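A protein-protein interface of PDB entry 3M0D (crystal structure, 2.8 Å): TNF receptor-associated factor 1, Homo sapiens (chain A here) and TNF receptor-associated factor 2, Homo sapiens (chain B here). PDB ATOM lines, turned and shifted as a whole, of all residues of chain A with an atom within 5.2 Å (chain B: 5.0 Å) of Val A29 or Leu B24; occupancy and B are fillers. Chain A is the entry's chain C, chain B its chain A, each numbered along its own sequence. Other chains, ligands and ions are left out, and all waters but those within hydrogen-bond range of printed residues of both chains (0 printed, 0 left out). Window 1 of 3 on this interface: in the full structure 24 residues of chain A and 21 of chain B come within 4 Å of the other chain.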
ATOM      1  N   VAL A  22     -12.952  29.821   3.835  1.00  0.00           N
ATOM      2  CA  VAL A  22     -14.167  29.120   3.441  1.00  0.00           C
ATOM      3  C   VAL A  22     -14.224  27.639   3.919  1.00  0.00           C
ATOM      4  O   VAL A  22     -15.285  27.138   4.292  1.00  0.00           O
ATOM      5  CB  VAL A  22     -14.389  29.236   1.922  1.00  0.00           C
ATOM      6  CG1 VAL A  22     -15.371  28.205   1.462  1.00  0.00           C
ATOM      7  CG2 VAL A  22     -14.892  30.606   1.565  1.00  0.00           C
ATOM      8  N   VAL A  24     -12.936  26.507   6.721  1.00  0.00           N
ATOM      9  CA  VAL A  24     -13.285  26.667   8.113  1.00  0.00           C
ATOM     10  C   VAL A  24     -14.770  26.993   8.248  1.00  0.00           C
ATOM     11  O   VAL A  24     -15.480  26.346   9.005  1.00  0.00           O
ATOM     12  CB  VAL A  24     -12.425  27.777   8.710  1.00  0.00           C
ATOM     13  CG1 VAL A  24     -12.617  27.870  10.182  1.00  0.00           C
ATOM     14  CG2 VAL A  24     -10.965  27.498   8.400  1.00  0.00           C
ATOM     15  N   LEU A  25     -15.234  27.991   7.504  1.00  0.00           N
ATOM     16  CA  LEU A  25     -16.648  28.356   7.509  1.00  0.00           C
ATOM     17  C   LEU A  25     -17.514  27.148   7.188  1.00  0.00           C
ATOM     18  O   LEU A  25     -18.545  26.907   7.836  1.00  0.00           O
ATOM     19  CB  LEU A  25     -16.940  29.493   6.522  1.00  0.00           C
ATOM     20  CG  LEU A  25     -16.442  30.881   6.939  1.00  0.00           C
ATOM     21  CD1 LEU A  25     -17.102  31.965   6.123  1.00  0.00           C
ATOM     22  CD2 LEU A  25     -16.708  31.136   8.388  1.00  0.00           C
ATOM     23  N   ASN A  26     -17.090  26.392   6.178  1.00  0.00           N
ATOM     24  CA  ASN A  26     -17.749  25.142   5.837  1.00  0.00           C
ATOM     25  C   ASN A  26     -17.870  24.229   7.058  1.00  0.00           C
ATOM     26  O   ASN A  26     -18.948  23.710   7.353  1.00  0.00           O
ATOM     27  CB  ASN A  26     -17.001  24.447   4.721  1.00  0.00           C
ATOM     28  CG  ASN A  26     -17.518  23.061   4.464  1.00  0.00           C
ATOM     29  OD1 ASN A  26     -18.700  22.874   4.149  1.00  0.00           O
ATOM     30  ND2 ASN A  26     -16.638  22.068   4.583  1.00  0.00           N
ATOM     31  N   LYS A  27     -16.769  24.058   7.786  1.00  0.00           N
ATOM     32  CA  LYS A  27     -16.781  23.260   9.014  1.00  0.00           C
ATOM     33  C   LYS A  27     -17.733  23.804  10.071  1.00  0.00           C
ATOM     34  O   LYS A  27     -18.403  23.048  10.765  1.00  0.00           O
ATOM     35  CB  LYS A  27     -15.384  23.169   9.621  1.00  0.00           C
ATOM     36  CG  LYS A  27     -14.459  22.207   8.914  1.00  0.00           C
ATOM     37  CD  LYS A  27     -13.088  22.239   9.555  1.00  0.00           C
ATOM     38  CE  LYS A  27     -12.290  20.993   9.217  1.00  0.00           C
ATOM     39  NZ  LYS A  27     -10.880  21.152   9.659  1.00  0.00           N
ATOM     40  N   GLU A  28     -17.771  25.124  10.199  1.00  0.00           N
ATOM     41  CA  GLU A  28     -18.606  25.759  11.198  1.00  0.00           C
ATOM     42  C   GLU A  28     -20.071  25.449  10.933  1.00  0.00           C
ATOM     43  O   GLU A  28     -20.798  25.001  11.824  1.00  0.00           O
ATOM     44  CB  GLU A  28     -18.381  27.262  11.179  1.00  0.00           C
ATOM     45  CG  GLU A  28     -18.916  27.973  12.402  1.00  0.00           C
ATOM     46  CD  GLU A  28     -18.421  29.387  12.481  1.00  0.00           C
ATOM     47  OE1 GLU A  28     -17.503  29.730  11.695  1.00  0.00           O
ATOM     48  OE2 GLU A  28     -18.949  30.155  13.321  1.00  0.00           O
ATOM     49  N   VAL A  29     -20.488  25.689   9.696  1.00  0.00           N
ATOM     50  CA  VAL A  29     -21.848  25.413   9.256  1.00  0.00           C
ATOM     51  C   VAL A  29     -22.262  23.955   9.564  1.00  0.00           C
ATOM     52  O   VAL A  29     -23.420  23.679   9.904  1.00  0.00           O
ATOM     53  CB  VAL A  29     -22.005  25.742   7.730  1.00  0.00           C
ATOM     54  CG1 VAL A  29     -23.238  25.099   7.141  1.00  0.00           C
ATOM     55  CG2 VAL A  29     -22.067  27.229   7.504  1.00  0.00           C
ATOM     56  N   GLU A  30     -21.307  23.035   9.461  1.00  0.00           N
ATOM     57  CA  GLU A  30     -21.586  21.619   9.621  1.00  0.00           C
ATOM     58  C   GLU A  30     -21.874  21.239  11.082  1.00  0.00           C
ATOM     59  O   GLU A  30     -22.854  20.556  11.385  1.00  0.00           O
ATOM     60  CB  GLU A  30     -20.413  20.801   9.066  1.00  0.00           C
ATOM     61  CG  GLU A  30     -20.742  19.326   8.883  1.00  0.00           C
ATOM     62  CD  GLU A  30     -22.173  19.117   8.409  1.00  0.00           C
ATOM     63  OE1 GLU A  30     -22.587  19.834   7.464  1.00  0.00           O
ATOM     64  OE2 GLU A  30     -22.877  18.248   8.987  1.00  0.00           O
ATOM     65  N   ALA A  31     -20.994  21.677  11.976  1.00  0.00           N
ATOM     66  CA  ALA A  31     -21.195  21.545  13.412  1.00  0.00           C
ATOM     67  C   ALA A  31     -22.565  22.105  13.847  1.00  0.00           C
ATOM     68  O   ALA A  31     -23.208  21.559  14.750  1.00  0.00           O
ATOM     69  CB  ALA A  31     -20.056  22.247  14.163  1.00  0.00           C
ATOM     70  N   SER A  32     -22.987  23.204  13.216  1.00  0.00           N
ATOM     71  CA  SER A  32     -24.285  23.820  13.480  1.00  0.00           C
ATOM     72  C   SER A  32     -25.393  22.866  13.097  1.00  0.00           C
ATOM     73  O   SER A  32     -26.343  22.672  13.846  1.00  0.00           O
ATOM     74  CB  SER A  32     -24.460  25.129  12.692  1.00  0.00           C
ATOM     75  OG  SER A  32     -23.734  26.198  13.265  1.00  0.00           O
ATOM     76  N   HIS A  33     -25.250  22.278  11.916  1.00  0.00           N
ATOM     77  CA  HIS A  33     -26.215  21.332  11.361  1.00  0.00           C
ATOM     78  C   HIS A  33     -26.374  20.103  12.251  1.00  0.00           C
ATOM     79  O   HIS A  33     -27.481  19.612  12.454  1.00  0.00           O
ATOM     80  CB  HIS A  33     -25.767  20.896   9.963  1.00  0.00           C
ATOM     81  CG  HIS A  33     -26.897  20.552   9.042  1.00  0.00           C
ATOM     82  ND1 HIS A  33     -27.905  19.683   9.388  1.00  0.00           N
ATOM     83  CD2 HIS A  33     -27.165  20.952   7.777  1.00  0.00           C
ATOM     84  CE1 HIS A  33     -28.754  19.567   8.382  1.00  0.00           C
ATOM     85  NE2 HIS A  33     -28.326  20.327   7.391  1.00  0.00           N
ATOM     86  N   ILE B  20     -16.893  25.794  -4.247  1.00  0.00           N
ATOM     87  CA  ILE B  20     -16.995  25.709  -2.799  1.00  0.00           C
ATOM     88  C   ILE B  20     -18.028  26.695  -2.243  1.00  0.00           C
ATOM     89  O   ILE B  20     -18.925  26.330  -1.474  1.00  0.00           O
ATOM     90  CB  ILE B  20     -15.649  26.066  -2.135  1.00  0.00           C
ATOM     91  CG1 ILE B  20     -14.465  25.550  -2.956  1.00  0.00           C
ATOM     92  CG2 ILE B  20     -15.602  25.567  -0.690  1.00  0.00           C
ATOM     93  CD1 ILE B  20     -13.112  25.862  -2.321  1.00  0.00           C
ATOM     94  N   VAL B  21     -17.881  27.956  -2.621  1.00  0.00           N
ATOM     95  CA  VAL B  21     -18.728  29.004  -2.076  1.00  0.00           C
ATOM     96  C   VAL B  21     -20.184  28.760  -2.444  1.00  0.00           C
ATOM     97  O   VAL B  21     -21.090  28.998  -1.642  1.00  0.00           O
ATOM     98  CB  VAL B  21     -18.268  30.400  -2.540  1.00  0.00           C
ATOM     99  CG1 VAL B  21     -19.303  31.453  -2.175  1.00  0.00           C
ATOM    100  CG2 VAL B  21     -16.917  30.728  -1.922  1.00  0.00           C
ATOM    101  N   CYS B  22     -20.396  28.277  -3.660  1.00  0.00           N
ATOM    102  CA  CYS B  22     -21.729  27.917  -4.115  1.00  0.00           C
ATOM    103  C   CYS B  22     -22.436  26.992  -3.117  1.00  0.00           C
ATOM    104  O   CYS B  22     -23.528  27.294  -2.645  1.00  0.00           O
ATOM    105  CB  CYS B  22     -21.634  27.229  -5.475  1.00  0.00           C
ATOM    106  SG  CYS B  22     -23.197  26.627  -6.087  1.00  0.00           S
ATOM    107  N   VAL B  23     -21.780  25.878  -2.795  1.00  0.00           N
ATOM    108  CA  VAL B  23     -22.314  24.843  -1.922  1.00  0.00           C
ATOM    109  C   VAL B  23     -22.460  25.319  -0.477  1.00  0.00           C
ATOM    110  O   VAL B  23     -23.460  25.033   0.199  1.00  0.00           O
ATOM    111  CB  VAL B  23     -21.395  23.581  -1.905  1.00  0.00           C
ATOM    112  CG1 VAL B  23     -21.938  22.532  -0.938  1.00  0.00           C
ATOM    113  CG2 VAL B  23     -21.256  22.982  -3.283  1.00  0.00           C
ATOM    114  N   LEU B  24     -21.441  26.019   0.006  1.00  0.00           N
ATOM    115  CA  LEU B  24     -21.498  26.557   1.353  1.00  0.00           C
ATOM    116  C   LEU B  24     -22.746  27.399   1.522  1.00  0.00           C
ATOM    117  O   LEU B  24     -23.492  27.203   2.480  1.00  0.00           O
ATOM    118  CB  LEU B  24     -20.270  27.396   1.656  1.00  0.00           C
ATOM    119  CG  LEU B  24     -20.284  28.032   3.034  1.00  0.00           C
ATOM    120  CD1 LEU B  24     -20.523  26.972   4.111  1.00  0.00           C
ATOM    121  CD2 LEU B  24     -18.982  28.787   3.263  1.00  0.00           C
ATOM    122  N   ASN B  25     -22.981  28.321   0.599  1.00  0.00           N
ATOM    123  CA  ASN B  25     -24.164  29.155   0.671  1.00  0.00           C
ATOM    124  C   ASN B  25     -25.456  28.361   0.726  1.00  0.00           C
ATOM    125  O   ASN B  25     -26.368  28.688   1.494  1.00  0.00           O
ATOM    126  CB  ASN B  25     -24.231  30.109  -0.515  1.00  0.00           C
ATOM    127  CG  ASN B  25     -23.485  31.386  -0.274  1.00  0.00           C
ATOM    128  OD1 ASN B  25     -22.764  31.853  -1.142  1.00  0.00           O
ATOM    129  ND2 ASN B  25     -23.622  31.942   0.912  1.00  0.00           N
ATOM    130  N   ARG B  26     -25.542  27.336  -0.112  1.00  0.00           N
ATOM    131  CA  ARG B  26     -26.728  26.500  -0.142  1.00  0.00           C
ATOM    132  C   ARG B  26     -26.950  25.911   1.254  1.00  0.00           C
ATOM    133  O   ARG B  26     -28.063  25.936   1.761  1.00  0.00           O
ATOM    134  CB  ARG B  26     -26.615  25.406  -1.219  1.00  0.00           C
ATOM    135  CG  ARG B  26     -27.903  24.625  -1.517  1.00  0.00           C
ATOM    136  CD  ARG B  26     -29.044  25.529  -1.985  1.00  0.00           C
ATOM    137  NE  ARG B  26     -30.360  24.868  -2.023  1.00  0.00           N
ATOM    138  CZ  ARG B  26     -31.132  24.650  -0.949  1.00  0.00           C
ATOM    139  NH1 ARG B  26     -30.733  25.006   0.268  1.00  0.00           N
ATOM    140  NH2 ARG B  26     -32.304  24.059  -1.087  1.00  0.00           N
ATOM    141  N   GLU B  27     -25.892  25.410   1.890  1.00  0.00           N
ATOM    142  CA  GLU B  27     -26.044  24.758   3.195  1.00  0.00           C
ATOM    143  C   GLU B  27     -26.413  25.723   4.305  1.00  0.00           C
ATOM    144  O   GLU B  27     -27.241  25.403   5.153  1.00  0.00           O
ATOM    145  CB  GLU B  27     -24.815  23.937   3.576  1.00  0.00           C
ATOM    146  CG  GLU B  27     -24.555  22.734   2.656  1.00  0.00           C
ATOM    147  CD  GLU B  27     -25.759  21.800   2.489  1.00  0.00           C
ATOM    148  OE1 GLU B  27     -26.490  21.553   3.483  1.00  0.00           O
ATOM    149  OE2 GLU B  27     -25.967  21.313   1.351  1.00  0.00           O
ATOM    150  N   VAL B  28     -25.821  26.912   4.295  1.00  0.00           N
ATOM    151  CA  VAL B  28     -26.258  27.958   5.212  1.00  0.00           C
ATOM    152  C   VAL B  28     -27.772  28.131   5.110  1.00  0.00           C
ATOM    153  O   VAL B  28     -28.471  28.183   6.121  1.00  0.00           O
ATOM    154  CB  VAL B  28     -25.564  29.294   4.920  1.00  0.00           C
ATOM    155  CG1 VAL B  28     -26.155  30.403   5.776  1.00  0.00           C
ATOM    156  CG2 VAL B  28     -24.093  29.169   5.201  1.00  0.00           C
ATOM    157  N   VAL B  31     -29.553  25.204   6.698  1.00  0.00           N
ATOM    158  CA  VAL B  31     -29.450  25.317   8.153  1.00  0.00           C
ATOM    159  C   VAL B  31     -30.385  26.419   8.668  1.00  0.00           C
ATOM    160  O   VAL B  31     -31.100  26.233   9.658  1.00  0.00           O
ATOM    161  CB  VAL B  31     -27.994  25.569   8.639  1.00  0.00           C
ATOM    162  CG1 VAL B  31     -27.983  26.020  10.092  1.00  0.00           C
ATOM    163  CG2 VAL B  31     -27.125  24.318   8.473  1.00  0.00           C
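Val A24 touches none of the printed residues of chain B.
Of the printed residues of chain B, Leu A25 touches Leu B24.
Of the printed residues of chain B, Asn A26 touches Leu B24.
Val A29 touches two residues of chain B.
Leu B24 touches three residues of chain A.
Of the printed residues of chain A, Val B31 touches His A33.
The nearest residue of chain A that does not touch Leu B24 is Val A22 (4.1 Å).
The nearest printed residue of chain B that does not touch Asn A26 is Ile B20 (5.7 Å).
Val A22 touches Ile B20.
CB of Leu A25 touches CD2 of Leu B24 (3.9 Å).
CD1 of Leu B24 touches CA of Asn A26, at 3.7 Å.
Leu B24 touches Val A29.
Val B28 touches Val A29 (CG2 to CG2, 3.6 Å).
Val B31 touches His A33.
Printed residues of chain B that touch a printed residue of chain A: Ile B20, Leu B24, Val B28 and Val B31.
Hydrophobic or aromatic side chains of chain B within 4 Å of the printed part of chain A: Ile B20, Leu B24, Val B28 and Val B31.
Of the 11 printed residues of chain A, 5 touch a printed residue of chain B.
Hydrophobic or aromatic side chains of chain A that line the printed part of chain B: Val A22, Leu A25, Val A29 and His A33.
Among the printed residues, no Asp or Glu carboxylate lies within 4 Å of a Lys or Arg side-chain nitrogen of the other chain.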
